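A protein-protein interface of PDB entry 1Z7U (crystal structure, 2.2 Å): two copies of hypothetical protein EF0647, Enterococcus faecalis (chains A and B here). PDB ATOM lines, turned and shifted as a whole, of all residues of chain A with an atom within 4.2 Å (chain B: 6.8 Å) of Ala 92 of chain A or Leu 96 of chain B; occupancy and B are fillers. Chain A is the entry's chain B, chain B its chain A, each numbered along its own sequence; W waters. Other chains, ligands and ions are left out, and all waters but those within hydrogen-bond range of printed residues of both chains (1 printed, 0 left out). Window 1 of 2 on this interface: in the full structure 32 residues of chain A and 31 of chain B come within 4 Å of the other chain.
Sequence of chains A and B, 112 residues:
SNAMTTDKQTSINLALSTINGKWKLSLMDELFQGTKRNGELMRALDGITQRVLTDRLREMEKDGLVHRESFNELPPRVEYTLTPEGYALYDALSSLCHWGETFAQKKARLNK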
ATOM      1  N   SER A  11      22.834  -4.328 -30.107  1.00  0.00           N
ATOM      2  CA  SER A  11      23.647  -4.116 -28.902  1.00  0.00           C
ATOM      3  C   SER A  11      23.510  -5.222 -27.892  1.00  0.00           C
ATOM      4  O   SER A  11      24.505  -5.619 -27.300  1.00  0.00           O
ATOM      5  CB  SER A  11      23.375  -2.784 -28.224  1.00  0.00           C
ATOM      6  OG  SER A  11      23.441  -1.756 -29.170  1.00  0.00           O
ATOM      7  N   ILE A  12      22.283  -5.710 -27.707  1.00  0.00           N
ATOM      8  CA  ILE A  12      22.011  -6.828 -26.808  1.00  0.00           C
ATOM      9  C   ILE A  12      22.687  -8.115 -27.306  1.00  0.00           C
ATOM     10  O   ILE A  12      23.351  -8.807 -26.541  1.00  0.00           O
ATOM     11  CB  ILE A  12      20.489  -7.033 -26.561  1.00  0.00           C
ATOM     12  CG1 ILE A  12      19.912  -5.865 -25.744  1.00  0.00           C
ATOM     13  CG2 ILE A  12      20.233  -8.354 -25.810  1.00  0.00           C
ATOM     14  CD1 ILE A  12      18.376  -5.781 -25.755  1.00  0.00           C
ATOM     15  N   ALA A  15      26.501  -7.954 -26.630  1.00  0.00           N
ATOM     16  CA  ALA A  15      26.828  -8.214 -25.242  1.00  0.00           C
ATOM     17  C   ALA A  15      26.746  -9.712 -24.964  1.00  0.00           C
ATOM     18  O   ALA A  15      27.677 -10.278 -24.426  1.00  0.00           O
ATOM     19  CB  ALA A  15      25.921  -7.430 -24.307  1.00  0.00           C
ATOM     20  N   ALA A  88      30.483  -4.529 -15.076  1.00  0.00           N
ATOM     21  CA  ALA A  88      29.292  -3.904 -15.643  1.00  0.00           C
ATOM     22  C   ALA A  88      28.432  -4.923 -16.383  1.00  0.00           C
ATOM     23  O   ALA A  88      27.226  -4.914 -16.227  1.00  0.00           O
ATOM     24  CB  ALA A  88      29.680  -2.739 -16.558  1.00  0.00           C
ATOM     25  N   LEU A  89      29.056  -5.798 -17.175  1.00  0.00           N
ATOM     26  CA  LEU A  89      28.349  -6.867 -17.872  1.00  0.00           C
ATOM     27  C   LEU A  89      27.784  -7.896 -16.906  1.00  0.00           C
ATOM     28  O   LEU A  89      26.648  -8.353 -17.076  1.00  0.00           O
ATOM     29  CB  LEU A  89      29.234  -7.540 -18.943  1.00  0.00           C
ATOM     30  CG  LEU A  89      28.560  -8.622 -19.807  1.00  0.00           C
ATOM     31  CD1 LEU A  89      27.316  -8.114 -20.605  1.00  0.00           C
ATOM     32  CD2 LEU A  89      29.545  -9.323 -20.742  1.00  0.00           C
ATOM     33  N   TYR A  90      28.566  -8.254 -15.890  1.00  0.00           N
ATOM     34  CA  TYR A  90      28.084  -9.131 -14.819  1.00  0.00           C
ATOM     35  C   TYR A  90      26.814  -8.593 -14.103  1.00  0.00           C
ATOM     36  O   TYR A  90      25.874  -9.366 -13.850  1.00  0.00           O
ATOM     37  CB  TYR A  90      29.213  -9.438 -13.827  1.00  0.00           C
ATOM     38  CG  TYR A  90      28.783 -10.251 -12.635  1.00  0.00           C
ATOM     39  CD1 TYR A  90      29.087 -11.601 -12.547  1.00  0.00           C
ATOM     40  CD2 TYR A  90      28.078  -9.668 -11.588  1.00  0.00           C
ATOM     41  CE1 TYR A  90      28.692 -12.350 -11.443  1.00  0.00           C
ATOM     42  CE2 TYR A  90      27.663 -10.418 -10.482  1.00  0.00           C
ATOM     43  CZ  TYR A  90      27.985 -11.748 -10.424  1.00  0.00           C
ATOM     44  OH  TYR A  90      27.599 -12.491  -9.328  1.00  0.00           O
ATOM     45  N   ASP A  91      26.802  -7.292 -13.799  1.00  0.00           N
ATOM     46  CA  ASP A  91      25.645  -6.640 -13.172  1.00  0.00           C
ATOM     47  C   ASP A  91      24.410  -6.751 -14.065  1.00  0.00           C
ATOM     48  O   ASP A  91      23.324  -7.078 -13.602  1.00  0.00           O
ATOM     49  CB  ASP A  91      25.938  -5.163 -12.879  1.00  0.00           C
ATOM     50  CG  ASP A  91      26.961  -4.958 -11.761  1.00  0.00           C
ATOM     51  OD1 ASP A  91      27.287  -5.918 -11.023  1.00  0.00           O
ATOM     52  OD2 ASP A  91      27.446  -3.811 -11.619  1.00  0.00           O
ATOM     53  N   ALA A  92      24.599  -6.487 -15.354  1.00  0.00           N
ATOM     54  CA  ALA A  92      23.528  -6.524 -16.339  1.00  0.00           C
ATOM     55  C   ALA A  92      22.978  -7.947 -16.538  1.00  0.00           C
ATOM     56  O   ALA A  92      21.763  -8.147 -16.621  1.00  0.00           O
ATOM     57  CB  ALA A  92      24.026  -5.926 -17.660  1.00  0.00           C
ATOM     58  N   LEU A  93      23.863  -8.937 -16.591  1.00  0.00           N
ATOM     59  CA  LEU A  93      23.427 -10.322 -16.628  1.00  0.00           C
ATOM     60  C   LEU A  93      22.737 -10.766 -15.345  1.00  0.00           C
ATOM     61  O   LEU A  93      21.803 -11.572 -15.405  1.00  0.00           O
ATOM     62  CB  LEU A  93      24.580 -11.258 -16.960  1.00  0.00           C
ATOM     63  CG  LEU A  93      25.232 -11.058 -18.328  1.00  0.00           C
ATOM     64  CD1 LEU A  93      26.647 -11.664 -18.330  1.00  0.00           C
ATOM     65  CD2 LEU A  93      24.354 -11.625 -19.444  1.00  0.00           C
ATOM     66  N   SER A  94      23.177 -10.240 -14.192  1.00  0.00           N
ATOM     67  CA  SER A  94      22.506 -10.549 -12.914  1.00  0.00           C
ATOM     68  C   SER A  94      21.053 -10.103 -12.855  1.00  0.00           C
ATOM     69  O   SER A  94      20.223 -10.789 -12.264  1.00  0.00           O
ATOM     70  CB  SER A  94      23.243  -9.948 -11.723  1.00  0.00           C
ATOM     71  OG  SER A  94      24.525 -10.522 -11.615  1.00  0.00           O
ATOM     72  N   SER A  95      20.770  -8.946 -13.445  1.00  0.00           N
ATOM     73  CA  SER A  95      19.426  -8.380 -13.510  1.00  0.00           C
ATOM     74  C   SER A  95      18.532  -9.232 -14.383  1.00  0.00           C
ATOM     75  O   SER A  95      17.385  -9.487 -14.031  1.00  0.00           O
ATOM     76  CB  SER A  95      19.477  -6.961 -14.064  1.00  0.00           C
ATOM     77  OG  SER A  95      20.170  -6.117 -13.172  1.00  0.00           O
ATOM     78  N   LEU A  96      19.079  -9.665 -15.517  1.00  0.00           N
ATOM     79  CA  LEU A  96      18.434 -10.616 -16.410  1.00  0.00           C
ATOM     80  C   LEU A  96      18.173 -11.952 -15.685  1.00  0.00           C
ATOM     81  O   LEU A  96      17.066 -12.459 -15.693  1.00  0.00           O
ATOM     82  CB  LEU A  96      19.334 -10.843 -17.626  1.00  0.00           C
ATOM     83  CG  LEU A  96      18.869 -10.886 -19.081  1.00  0.00           C
ATOM     84  CD1 LEU A  96      19.724 -11.884 -19.879  1.00  0.00           C
ATOM     85  CD2 LEU A  96      17.370 -11.153 -19.282  1.00  0.00           C
ATOM     86  N   LEU B  16      15.400 -14.612 -21.291  1.00  0.00           N
ATOM     87  CA  LEU B  16      15.507 -14.221 -22.706  1.00  0.00           C
ATOM     88  C   LEU B  16      14.400 -14.807 -23.581  1.00  0.00           C
ATOM     89  O   LEU B  16      13.943 -14.170 -24.524  1.00  0.00           O
ATOM     90  CB  LEU B  16      16.884 -14.570 -23.286  1.00  0.00           C
ATOM     91  CG  LEU B  16      18.130 -13.795 -22.842  1.00  0.00           C
ATOM     92  CD1 LEU B  16      19.389 -14.538 -23.271  1.00  0.00           C
ATOM     93  CD2 LEU B  16      18.142 -12.336 -23.371  1.00  0.00           C
ATOM     94  N   ASP B  91      14.578  -2.602 -18.057  1.00  0.00           N
ATOM     95  CA  ASP B  91      15.791  -2.052 -17.430  1.00  0.00           C
ATOM     96  C   ASP B  91      17.025  -2.950 -17.539  1.00  0.00           C
ATOM     97  O   ASP B  91      18.127  -2.454 -17.781  1.00  0.00           O
ATOM     98  CB  ASP B  91      15.535  -1.758 -15.950  1.00  0.00           C
ATOM     99  CG  ASP B  91      14.634  -0.542 -15.727  1.00  0.00           C
ATOM    100  OD1 ASP B  91      14.368   0.232 -16.687  1.00  0.00           O
ATOM    101  OD2 ASP B  91      14.210  -0.352 -14.558  1.00  0.00           O
ATOM    102  N   ALA B  92      16.841  -4.256 -17.335  1.00  0.00           N
ATOM    103  CA  ALA B  92      17.919  -5.248 -17.506  1.00  0.00           C
ATOM    104  C   ALA B  92      18.409  -5.275 -18.945  1.00  0.00           C
ATOM    105  O   ALA B  92      19.611  -5.331 -19.194  1.00  0.00           O
ATOM    106  CB  ALA B  92      17.455  -6.654 -17.078  1.00  0.00           C
ATOM    107  N   LEU B  93      17.473  -5.246 -19.891  1.00  0.00           N
ATOM    108  CA  LEU B  93      17.828  -5.207 -21.314  1.00  0.00           C
ATOM    109  C   LEU B  93      18.516  -3.909 -21.737  1.00  0.00           C
ATOM    110  O   LEU B  93      19.419  -3.938 -22.588  1.00  0.00           O
ATOM    111  CB  LEU B  93      16.611  -5.499 -22.197  1.00  0.00           C
ATOM    112  CG  LEU B  93      16.023  -6.918 -22.123  1.00  0.00           C
ATOM    113  CD1 LEU B  93      14.836  -7.052 -23.071  1.00  0.00           C
ATOM    114  CD2 LEU B  93      17.054  -7.987 -22.427  1.00  0.00           C
ATOM    115  N   SER B  94      18.093  -2.782 -21.152  1.00  0.00           N
ATOM    116  CA  SER B  94      18.732  -1.480 -21.424  1.00  0.00           C
ATOM    117  C   SER B  94      20.161  -1.438 -20.920  1.00  0.00           C
ATOM    118  O   SER B  94      21.011  -0.851 -21.567  1.00  0.00           O
ATOM    119  CB  SER B  94      17.956  -0.311 -20.802  1.00  0.00           C
ATOM    120  OG  SER B  94      16.718  -0.148 -21.440  1.00  0.00           O
ATOM    121  N   SER B  95      20.416  -2.058 -19.770  1.00  0.00           N
ATOM    122  CA  SER B  95      21.783  -2.203 -19.231  1.00  0.00           C
ATOM    123  C   SER B  95      22.706  -3.001 -20.152  1.00  0.00           C
ATOM    124  O   SER B  95      23.837  -2.594 -20.374  1.00  0.00           O
ATOM    125  CB  SER B  95      21.748  -2.850 -17.852  1.00  0.00           C
ATOM    126  OG  SER B  95      21.042  -2.028 -16.945  1.00  0.00           O
ATOM    127  N   LEU B  96      22.223  -4.132 -20.673  1.00  0.00           N
ATOM    128  CA  LEU B  96      22.935  -4.923 -21.682  1.00  0.00           C
ATOM    129  C   LEU B  96      23.136  -4.146 -22.972  1.00  0.00           C
ATOM    130  O   LEU B  96      24.201  -4.191 -23.602  1.00  0.00           O
ATOM    131  CB  LEU B  96      22.131  -6.176 -22.051  1.00  0.00           C
ATOM    132  CG  LEU B  96      22.124  -7.374 -21.125  1.00  0.00           C
ATOM    133  CD1 LEU B  96      21.396  -8.500 -21.825  1.00  0.00           C
ATOM    134  CD2 LEU B  96      23.560  -7.799 -20.786  1.00  0.00           C
ATOM    135  N   CYS B  97      22.081  -3.455 -23.385  1.00  0.00           N
ATOM    136  CA  CYS B  97      22.168  -2.621 -24.552  1.00  0.00           C
ATOM    137  C   CYS B  97      23.297  -1.608 -24.371  1.00  0.00           C
ATOM    138  O   CYS B  97      24.100  -1.420 -25.262  1.00  0.00           O
ATOM    139  CB  CYS B  97      20.838  -1.916 -24.801  1.00  0.00           C
ATOM    140  SG  CYS B  97      20.929  -0.784 -26.154  1.00  0.00           S
ATOM    141  N   HIS B  98      23.339  -0.971 -23.202  1.00  0.00           N
ATOM    142  CA  HIS B  98      24.321   0.054 -22.888  1.00  0.00           C
ATOM    143  C   HIS B  98      25.727  -0.563 -22.898  1.00  0.00           C
ATOM    144  O   HIS B  98      26.651  -0.014 -23.487  1.00  0.00           O
ATOM    145  CB  HIS B  98      23.983   0.675 -21.523  1.00  0.00           C
ATOM    146  CG  HIS B  98      24.662   1.983 -21.247  1.00  0.00           C
ATOM    147  ND1 HIS B  98      25.948   2.263 -21.653  1.00  0.00           N
ATOM    148  CD2 HIS B  98      24.252   3.065 -20.544  1.00  0.00           C
ATOM    149  CE1 HIS B  98      26.290   3.471 -21.244  1.00  0.00           C
ATOM    150  NE2 HIS B  98      25.279   3.979 -20.564  1.00  0.00           N
ATOM    151  N   TRP B  99      25.876  -1.730 -22.281  1.00  0.00           N
ATOM    152  CA  TRP B  99      27.118  -2.472 -22.387  1.00  0.00           C
ATOM    153  C   TRP B  99      27.568  -2.724 -23.845  1.00  0.00           C
ATOM    154  O   TRP B  99      28.722  -2.426 -24.207  1.00  0.00           O
ATOM    155  CB  TRP B  99      27.047  -3.797 -21.610  1.00  0.00           C
ATOM    156  CG  TRP B  99      28.400  -4.260 -21.311  1.00  0.00           C
ATOM    157  CD1 TRP B  99      29.136  -3.958 -20.211  1.00  0.00           C
ATOM    158  CD2 TRP B  99      29.248  -5.046 -22.167  1.00  0.00           C
ATOM    159  NE1 TRP B  99      30.383  -4.533 -20.306  1.00  0.00           N
ATOM    160  CE2 TRP B  99      30.474  -5.204 -21.501  1.00  0.00           C
ATOM    161  CE3 TRP B  99      29.084  -5.634 -23.424  1.00  0.00           C
ATOM    162  CZ2 TRP B  99      31.527  -5.918 -22.050  1.00  0.00           C
ATOM    163  CZ3 TRP B  99      30.131  -6.363 -23.964  1.00  0.00           C
ATOM    164  CH2 TRP B  99      31.334  -6.491 -23.281  1.00  0.00           C
ATOM    165  N   GLY B 100      26.684  -3.292 -24.666  1.00  0.00           N
ATOM    166  CA  GLY B 100      27.040  -3.615 -26.051  1.00  0.00           C
ATOM    167  C   GLY B 100      27.363  -2.406 -26.917  1.00  0.00           C
ATOM    168  O   GLY B 100      28.140  -2.489 -27.852  1.00  0.00           O
ATOM    169  N   GLU B 101      26.749  -1.276 -26.607  1.00  0.00           N
ATOM    170  CA  GLU B 101      27.000  -0.011 -27.285  1.00  0.00           C
ATOM    171  C   GLU B 101      28.423   0.470 -26.975  1.00  0.00           C
ATOM    172  O   GLU B 101      29.178   0.814 -27.870  1.00  0.00           O
ATOM    173  CB  GLU B 101      25.953   1.002 -26.796  1.00  0.00           C
ATOM    174  CG  GLU B 101      25.992   2.373 -27.426  1.00  0.00           C
ATOM    175  CD  GLU B 101      25.050   3.347 -26.724  1.00  0.00           C
ATOM    176  OE1 GLU B 101      23.940   3.593 -27.254  1.00  0.00           O
ATOM    177  OE2 GLU B 101      25.410   3.845 -25.623  1.00  0.00           O
HETATM  178  O   HOH W   1      20.880  -3.940 -14.795  1.00  0.00           O
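The backbone carbonyl oxygen of Asp 91 of chain B sits at hydrogen-bond distance from the side-chain hydroxyl of Ser 95 of chain B, at 3.1 Å. OG of Ser 95 of chain A lies within hydrogen-bond range of O of Asp 91 of chain A, at 3.3 Å.
Among the printed residues, merely in contact across the chains: Ser 11 of chain A with Cys 97 of chain B (3.3 Å), Ser 11 of chain A with Gly 100 of chain B (3.5 Å), Leu 89 of chain A with Trp 99 of chain B (3.5 Å), Ser 95 of chain A with Ala 92 of chain B (3.6 Å), Ala 92 of chain A with Leu 96 of chain B (3.7 Å), Ile 12 of chain A with Leu 93 of chain B (3.7 Å), Ala 15 of chain A with Leu 96 of chain B (3.7 Å), Ala 15 of chain A with Trp 99 of chain B (3.7 Å), Leu 96 of chain A with Ala 92 of chain B (3.8 Å), Leu 89 of chain A with Leu 96 of chain B (3.8 Å), Ala 92 of chain A with Ser 95 of chain B (3.8 Å), Leu 96 of chain A with Leu 16 of chain B (3.9 Å), Ala 88 of chain A with Trp 99 of chain B (3.9 Å) and Ser 11 of chain A with Leu 96 of chain B (3.98 Å).
Ala 92 of chain A touches Ser 95 of chain B, and with the chains exchanged Ser 95 of chain A touches Ala 92 of chain B. Ala 92 of chain A touches Leu 96 of chain B, and with the chains exchanged Leu 96 of chain A touches Ala 92 of chain B. Of the 14 pairs that touch across the chains among the printed residues, 4 have their exchanged pair printed and touching as well.
Water W1 bridges the side-chain hydroxyl (OG) of Ser 95 of chain A (2.8 Å) and the side-chain hydroxyl (OG) of Ser 95 of chain B (2.9 Å).
Printed residues of chain B within 4 Å of Ile 12 of chain A: Leu 93 (3.7 Å). Of chain B, only Ser 95 and Leu 96 come within 4 Å of Ala 92 of chain A. Of the printed residues of chain B, Ser 95 of chain A touches Ala 92. Printed residues of chain A within 4 Å of Ala 92 of chain B: Ser 95 (3.6 Å) and Leu 96 (3.8 Å). Printed residues of chain A within 4 Å of Leu 93 of chain B: Ile 12. Of the printed residues of chain A, Ser 95 of chain B touches Ala 92. Of chain A, only Ser 11, Ala 15, Leu 89 and Ala 92 come within 4 Å of Leu 96 of chain B. The nearest printed residue of chain B that does not touch Ile 12 of chain A is Cys 97 of chain B (4.01 Å).
Of the 12 printed residues of chain A, 8 touch a printed residue of chain B. Hydrophobic or aromatic side chains of chain A within 4 Å of the printed part of chain B: Ile 12, Ala 15, Ala 88, Leu 89, Ala 92 and Leu 96. Printed residues of chain B that touch a printed residue of chain A: Leu 16, Ala 92, Leu 93, Ser 95, Leu 96, Cys 97, Trp 99 and Gly 100. Hydrophobic or aromatic side chains of chain B that line the printed part of chain A: Leu 16, Ala 92, Leu 93, Leu 96 and Trp 99.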
